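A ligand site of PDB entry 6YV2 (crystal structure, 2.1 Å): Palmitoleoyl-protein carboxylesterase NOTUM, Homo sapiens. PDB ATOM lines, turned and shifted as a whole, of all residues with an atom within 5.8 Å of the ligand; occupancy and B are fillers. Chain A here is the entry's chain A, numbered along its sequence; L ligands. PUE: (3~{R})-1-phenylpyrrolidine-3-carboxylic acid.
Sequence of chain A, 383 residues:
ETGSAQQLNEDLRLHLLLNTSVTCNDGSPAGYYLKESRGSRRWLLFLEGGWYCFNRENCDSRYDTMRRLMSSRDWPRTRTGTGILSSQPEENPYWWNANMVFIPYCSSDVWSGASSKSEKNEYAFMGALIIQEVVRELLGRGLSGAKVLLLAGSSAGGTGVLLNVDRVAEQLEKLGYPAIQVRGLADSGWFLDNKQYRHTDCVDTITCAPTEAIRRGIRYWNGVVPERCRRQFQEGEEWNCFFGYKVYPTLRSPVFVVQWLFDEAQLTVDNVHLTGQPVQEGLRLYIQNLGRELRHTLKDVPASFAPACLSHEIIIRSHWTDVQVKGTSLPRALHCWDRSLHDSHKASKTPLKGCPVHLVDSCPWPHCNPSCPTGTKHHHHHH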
ATOM      1  N   GLY A  49      28.028  21.699   0.091  1.00  0.00           N
ATOM      2  CA  GLY A  49      27.250  20.571  -0.357  1.00  0.00           C
ATOM      3  C   GLY A  49      27.762  19.264   0.218  1.00  0.00           C
ATOM      4  O   GLY A  49      28.637  19.223   1.087  1.00  0.00           O
ATOM      5  N   GLY A  50      27.190  18.172  -0.285  1.00  0.00           N
ATOM      6  CA  GLY A  50      27.610  16.861   0.172  1.00  0.00           C
ATOM      7  C   GLY A  50      26.489  15.846   0.302  1.00  0.00           C
ATOM      8  O   GLY A  50      26.422  15.122   1.291  1.00  0.00           O
ATOM      9  N   TRP A  51      25.616  15.805  -0.706  1.00  0.00           N
ATOM     10  CA  TRP A  51      24.513  14.825  -0.784  1.00  0.00           C
ATOM     11  C   TRP A  51      23.623  15.000   0.450  1.00  0.00           C
ATOM     12  O   TRP A  51      23.314  16.134   0.832  1.00  0.00           O
ATOM     13  CB  TRP A  51      25.075  13.433  -0.969  1.00  0.00           C
ATOM     14  CG  TRP A  51      25.610  13.172  -2.349  1.00  0.00           C
ATOM     15  CD1 TRP A  51      26.858  13.456  -2.811  1.00  0.00           C
ATOM     16  CD2 TRP A  51      24.896  12.577  -3.442  1.00  0.00           C
ATOM     17  NE1 TRP A  51      26.971  13.073  -4.130  1.00  0.00           N
ATOM     18  CE2 TRP A  51      25.786  12.534  -4.538  1.00  0.00           C
ATOM     19  CE3 TRP A  51      23.603  12.085  -3.602  1.00  0.00           C
ATOM     20  CZ2 TRP A  51      25.406  12.013  -5.780  1.00  0.00           C
ATOM     21  CZ3 TRP A  51      23.236  11.567  -4.826  1.00  0.00           C
ATOM     22  CH2 TRP A  51      24.131  11.531  -5.894  1.00  0.00           C
ATOM     23  N   TYR A  52      23.200  13.906   1.074  1.00  0.00           N
ATOM     24  CA  TYR A  52      22.214  13.906   2.155  1.00  0.00           C
ATOM     25  C   TYR A  52      22.073  12.491   2.694  1.00  0.00           C
ATOM     26  O   TYR A  52      22.793  11.584   2.262  1.00  0.00           O
ATOM     27  CB  TYR A  52      20.866  14.423   1.642  1.00  0.00           C
ATOM     28  CG  TYR A  52      20.524  13.920   0.254  1.00  0.00           C
ATOM     29  CD1 TYR A  52      20.151  12.591   0.047  1.00  0.00           C
ATOM     30  CD2 TYR A  52      20.600  14.763  -0.845  1.00  0.00           C
ATOM     31  CE1 TYR A  52      19.851  12.124  -1.221  1.00  0.00           C
ATOM     32  CE2 TYR A  52      20.298  14.294  -2.123  1.00  0.00           C
ATOM     33  CZ  TYR A  52      19.921  12.982  -2.301  1.00  0.00           C
ATOM     34  OH  TYR A  52      19.623  12.526  -3.562  1.00  0.00           O
ATOM     35  N   VAL A 110      19.811  18.819   2.971  1.00  0.00           N
ATOM     36  CA  VAL A 110      19.754  19.801   1.886  1.00  0.00           C
ATOM     37  C   VAL A 110      19.368  21.163   2.461  1.00  0.00           C
ATOM     38  O   VAL A 110      18.694  21.964   1.807  1.00  0.00           O
ATOM     39  CB  VAL A 110      18.799  19.348   0.764  1.00  0.00           C
ATOM     40  CG1 VAL A 110      19.110  20.082  -0.531  1.00  0.00           C
ATOM     41  CG2 VAL A 110      18.902  17.843   0.541  1.00  0.00           C
ATOM     42  N   SER A 154      26.947  25.176  -3.384  1.00  0.00           N
ATOM     43  CA  SER A 154      27.190  24.246  -4.474  1.00  0.00           C
ATOM     44  C   SER A 154      26.515  22.911  -4.178  1.00  0.00           C
ATOM     45  O   SER A 154      26.481  22.468  -3.027  1.00  0.00           O
ATOM     46  CB  SER A 154      28.682  24.024  -4.705  1.00  0.00           C
ATOM     47  OG  SER A 154      29.290  25.199  -5.224  1.00  0.00           O
ATOM     48  N   SER A 155      25.980  22.292  -5.226  1.00  0.00           N
ATOM     49  CA  SER A 155      25.264  21.025  -5.135  1.00  0.00           C
ATOM     50  C   SER A 155      24.164  21.100  -4.091  1.00  0.00           C
ATOM     51  O   SER A 155      23.231  21.896  -4.230  1.00  0.00           O
ATOM     52  CB  SER A 155      26.234  19.873  -4.843  1.00  0.00           C
ATOM     53  OG  SER A 155      26.918  20.058  -3.614  1.00  0.00           O
ATOM     54  N   ALA A 156      24.245  20.276  -3.034  1.00  0.00           N
ATOM     55  CA  ALA A 156      23.235  20.319  -1.989  1.00  0.00           C
ATOM     56  C   ALA A 156      23.118  21.721  -1.398  1.00  0.00           C
ATOM     57  O   ALA A 156      22.012  22.174  -1.058  1.00  0.00           O
ATOM     58  CB  ALA A 156      23.556  19.304  -0.893  1.00  0.00           C
ATOM     59  N   GLY A 157      24.244  22.433  -1.277  1.00  0.00           N
ATOM     60  CA  GLY A 157      24.196  23.823  -0.873  1.00  0.00           C
ATOM     61  C   GLY A 157      23.525  24.716  -1.900  1.00  0.00           C
ATOM     62  O   GLY A 157      22.869  25.699  -1.537  1.00  0.00           O
ATOM     63  N   THR A 159      20.998  23.815  -3.889  1.00  0.00           N
ATOM     64  CA  THR A 159      19.575  23.650  -3.598  1.00  0.00           C
ATOM     65  C   THR A 159      19.204  24.324  -2.284  1.00  0.00           C
ATOM     66  O   THR A 159      18.097  24.863  -2.160  1.00  0.00           O
ATOM     67  CB  THR A 159      19.225  22.160  -3.556  1.00  0.00           C
ATOM     68  OG1 THR A 159      19.779  21.500  -4.697  1.00  0.00           O
ATOM     69  CG2 THR A 159      17.710  21.972  -3.564  1.00  0.00           C
ATOM     70  N   SER A 188      24.958  24.145  -9.140  1.00  0.00           N
ATOM     71  CA  SER A 188      24.823  22.694  -9.280  1.00  0.00           C
ATOM     72  C   SER A 188      23.761  22.131  -8.344  1.00  0.00           C
ATOM     73  O   SER A 188      23.835  20.969  -7.940  1.00  0.00           O
ATOM     74  CB  SER A 188      26.162  21.991  -9.058  1.00  0.00           C
ATOM     75  OG  SER A 188      27.080  22.358 -10.061  1.00  0.00           O
ATOM     76  N   GLY A 189      22.756  22.941  -8.006  1.00  0.00           N
ATOM     77  CA  GLY A 189      21.649  22.476  -7.187  1.00  0.00           C
ATOM     78  C   GLY A 189      20.330  22.542  -7.930  1.00  0.00           C
ATOM     79  O   GLY A 189      19.268  22.585  -7.312  1.00  0.00           O
ATOM     80  N   PHE A 191      18.118  20.530 -10.151  1.00  0.00           N
ATOM     81  CA  PHE A 191      17.946  19.138 -10.536  1.00  0.00           C
ATOM     82  C   PHE A 191      16.591  18.913 -11.210  1.00  0.00           C
ATOM     83  O   PHE A 191      15.667  19.710 -11.112  1.00  0.00           O
ATOM     84  CB  PHE A 191      18.088  18.223  -9.326  1.00  0.00           C
ATOM     85  CG  PHE A 191      19.473  18.191  -8.747  1.00  0.00           C
ATOM     86  CD1 PHE A 191      20.434  17.350  -9.279  1.00  0.00           C
ATOM     87  CD2 PHE A 191      19.809  19.011  -7.686  1.00  0.00           C
ATOM     88  CE1 PHE A 191      21.710  17.320  -8.744  1.00  0.00           C
ATOM     89  CE2 PHE A 191      21.083  18.989  -7.163  1.00  0.00           C
ATOM     90  CZ  PHE A 191      22.044  18.148  -7.695  1.00  0.00           C
ATOM     91  N   PRO A 210      16.025  10.766  -8.071  1.00  0.00           N
ATOM     92  CA  PRO A 210      15.892  12.087  -7.429  1.00  0.00           C
ATOM     93  C   PRO A 210      14.522  12.333  -6.841  1.00  0.00           C
ATOM     94  O   PRO A 210      14.412  12.932  -5.755  1.00  0.00           O
ATOM     95  CB  PRO A 210      16.223  13.071  -8.563  1.00  0.00           C
ATOM     96  CG  PRO A 210      15.998  12.285  -9.828  1.00  0.00           C
ATOM     97  CD  PRO A 210      16.381  10.876  -9.499  1.00  0.00           C
ATOM     98  N   ILE A 214      14.013  12.794  -2.403  1.00  0.00           N
ATOM     99  CA  ILE A 214      13.484  13.970  -1.709  1.00  0.00           C
ATOM    100  C   ILE A 214      12.185  13.630  -0.987  1.00  0.00           C
ATOM    101  O   ILE A 214      11.921  14.143   0.113  1.00  0.00           O
ATOM    102  CB  ILE A 214      13.300  15.127  -2.705  1.00  0.00           C
ATOM    103  CG1 ILE A 214      14.638  15.517  -3.332  1.00  0.00           C
ATOM    104  CG2 ILE A 214      12.660  16.334  -2.020  1.00  0.00           C
ATOM    105  CD1 ILE A 214      15.747  15.789  -2.323  1.00  0.00           C
ATOM    106  N   PHE A 242      11.956  21.119  -3.747  1.00  0.00           N
ATOM    107  CA  PHE A 242      13.400  20.909  -3.785  1.00  0.00           C
ATOM    108  C   PHE A 242      13.968  20.948  -5.194  1.00  0.00           C
ATOM    109  O   PHE A 242      15.184  20.867  -5.364  1.00  0.00           O
ATOM    110  CB  PHE A 242      13.748  19.559  -3.140  1.00  0.00           C
ATOM    111  CG  PHE A 242      13.757  19.571  -1.638  1.00  0.00           C
ATOM    112  CD1 PHE A 242      12.616  19.883  -0.919  1.00  0.00           C
ATOM    113  CD2 PHE A 242      14.913  19.252  -0.936  1.00  0.00           C
ATOM    114  CE1 PHE A 242      12.624  19.888   0.460  1.00  0.00           C
ATOM    115  CE2 PHE A 242      14.932  19.247   0.443  1.00  0.00           C
ATOM    116  CZ  PHE A 242      13.787  19.565   1.141  1.00  0.00           C
ATOM    117  N   PHE A 243      13.113  21.069  -6.209  1.00  0.00           N
ATOM    118  CA  PHE A 243      13.550  21.054  -7.593  1.00  0.00           C
ATOM    119  C   PHE A 243      13.503  22.466  -8.160  1.00  0.00           C
ATOM    120  O   PHE A 243      12.464  23.125  -8.094  1.00  0.00           O
ATOM    121  CB  PHE A 243      12.698  20.081  -8.414  1.00  0.00           C
ATOM    122  CG  PHE A 243      12.918  18.648  -8.019  1.00  0.00           C
ATOM    123  CD1 PHE A 243      12.185  18.077  -6.995  1.00  0.00           C
ATOM    124  CD2 PHE A 243      13.898  17.888  -8.644  1.00  0.00           C
ATOM    125  CE1 PHE A 243      12.399  16.764  -6.615  1.00  0.00           C
ATOM    126  CE2 PHE A 243      14.122  16.584  -8.268  1.00  0.00           C
ATOM    127  CZ  PHE A 243      13.378  16.022  -7.254  1.00  0.00           C
ATOM    128  N   ASP A 263      25.113  17.496 -15.263  1.00  0.00           N
ATOM    129  CA  ASP A 263      25.705  17.395 -13.946  1.00  0.00           C
ATOM    130  C   ASP A 263      25.939  15.935 -13.579  1.00  0.00           C
ATOM    131  O   ASP A 263      25.060  15.093 -13.758  1.00  0.00           O
ATOM    132  CB  ASP A 263      24.801  18.061 -12.898  1.00  0.00           C
ATOM    133  CG  ASP A 263      25.471  18.210 -11.555  1.00  0.00           C
ATOM    134  OD1 ASP A 263      26.191  19.214 -11.351  1.00  0.00           O
ATOM    135  OD2 ASP A 263      25.292  17.316 -10.696  1.00  0.00           O
ATOM    136  N   ALA A 265      26.150  14.494 -10.699  1.00  0.00           N
ATOM    137  CA  ALA A 265      25.237  14.007  -9.681  1.00  0.00           C
ATOM    138  C   ALA A 265      23.854  13.731 -10.266  1.00  0.00           C
ATOM    139  O   ALA A 265      23.180  12.779  -9.856  1.00  0.00           O
ATOM    140  CB  ALA A 265      25.141  15.009  -8.530  1.00  0.00           C
ATOM    141  N   GLN A 266      23.416  14.555 -11.217  1.00  0.00           N
ATOM    142  CA  GLN A 266      22.149  14.286 -11.897  1.00  0.00           C
ATOM    143  C   GLN A 266      22.226  12.992 -12.701  1.00  0.00           C
ATOM    144  O   GLN A 266      21.276  12.199 -12.712  1.00  0.00           O
ATOM    145  CB  GLN A 266      21.776  15.455 -12.809  1.00  0.00           C
ATOM    146  CG  GLN A 266      20.549  15.204 -13.687  1.00  0.00           C
ATOM    147  CD  GLN A 266      19.229  15.398 -12.962  1.00  0.00           C
ATOM    148  OE1 GLN A 266      19.009  16.415 -12.311  1.00  0.00           O
ATOM    149  NE2 GLN A 266      18.342  14.406 -13.076  1.00  0.00           N
ATOM    150  N   VAL A 269      22.158   9.960 -10.050  1.00  0.00           N
ATOM    151  CA  VAL A 269      20.826   9.598  -9.576  1.00  0.00           C
ATOM    152  C   VAL A 269      19.958   9.071 -10.698  1.00  0.00           C
ATOM    153  O   VAL A 269      18.940   8.421 -10.437  1.00  0.00           O
ATOM    154  CB  VAL A 269      20.147  10.789  -8.870  1.00  0.00           C
ATOM    155  CG1 VAL A 269      20.935  11.206  -7.648  1.00  0.00           C
ATOM    156  CG2 VAL A 269      19.970  11.965  -9.830  1.00  0.00           C
ATOM    157  N   HIS A 312      30.851  18.554 -12.047  1.00  0.00           N
ATOM    158  CA  HIS A 312      30.115  18.690 -10.791  1.00  0.00           C
ATOM    159  C   HIS A 312      30.654  19.890 -10.036  1.00  0.00           C
ATOM    160  O   HIS A 312      31.810  19.897  -9.622  1.00  0.00           O
ATOM    161  CB  HIS A 312      30.237  17.419  -9.947  1.00  0.00           C
ATOM    162  CG  HIS A 312      29.353  17.414  -8.737  1.00  0.00           C
ATOM    163  ND1 HIS A 312      29.724  16.828  -7.546  1.00  0.00           N
ATOM    164  CD2 HIS A 312      28.103  17.899  -8.544  1.00  0.00           C
ATOM    165  CE1 HIS A 312      28.743  16.969  -6.662  1.00  0.00           C
ATOM    166  NE2 HIS A 312      27.746  17.608  -7.244  1.00  0.00           N
HETATM  167  C2  PUE L   1      22.741  15.045  -5.540  1.00  0.00           C
HETATM  168  C3  PUE L   1      21.230  14.912  -5.665  1.00  0.00           C
HETATM  169  C4  PUE L   1      21.760  16.850  -4.299  1.00  0.00           C
HETATM  170  C5  PUE L   1      19.433  16.605  -5.198  1.00  0.00           C
HETATM  171  C6  PUE L   1      19.051  17.798  -4.598  1.00  0.00           C
HETATM  172  C10 PUE L   1      18.505  15.885  -5.946  1.00  0.00           C
HETATM  173  N   PUE L   1      20.730  16.140  -5.061  1.00  0.00           N
HETATM  174  C   PUE L   1      24.298  16.601  -4.286  1.00  0.00           C
HETATM  175  O   PUE L   1      24.540  17.268  -3.186  1.00  0.00           O
HETATM  176  C1  PUE L   1      22.962  15.903  -4.269  1.00  0.00           C
HETATM  177  C7  PUE L   1      17.749  18.267  -4.766  1.00  0.00           C
HETATM  178  C8  PUE L   1      16.844  17.558  -5.509  1.00  0.00           C
HETATM  179  C9  PUE L   1      17.217  16.367  -6.098  1.00  0.00           C
HETATM  180  O1  PUE L   1      25.071  16.535  -5.221  1.00  0.00           O
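Residues that only touch the ligand: Tyr 52, Ser 155, Thr 159, Phe 191, Ile 214, Phe 242, Phe 243, Ala 265 and His 312. Hydrophobic or aromatic side chains within 4 Å of the ligand: Trp 51, Tyr 52, Ala 156, Phe 191, Ile 214, Phe 243, Ala 265 and His 312. 11 residues have an atom within 4 Å of the ligand: Trp 51, Tyr 52, Ser 155, Ala 156, Thr 159, Phe 191, Ile 214, Phe 242, Phe 243, Ala 265 and His 312.
The backbone NH (N) of Ala 156 sits at hydrogen-bond distance from an oxygen (O) of the ligand. The backbone NH (N) of Trp 51 is in hydrogen-bond range of an oxygen (O) of the ligand, at 3.1 Å.
N of Ala 265 is in hydrogen-bond range of OD2 of Asp 263 (2.9 Å). O of Gly 189 is in hydrogen-bond range of OG1 of Thr 159, 2.9 Å away.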
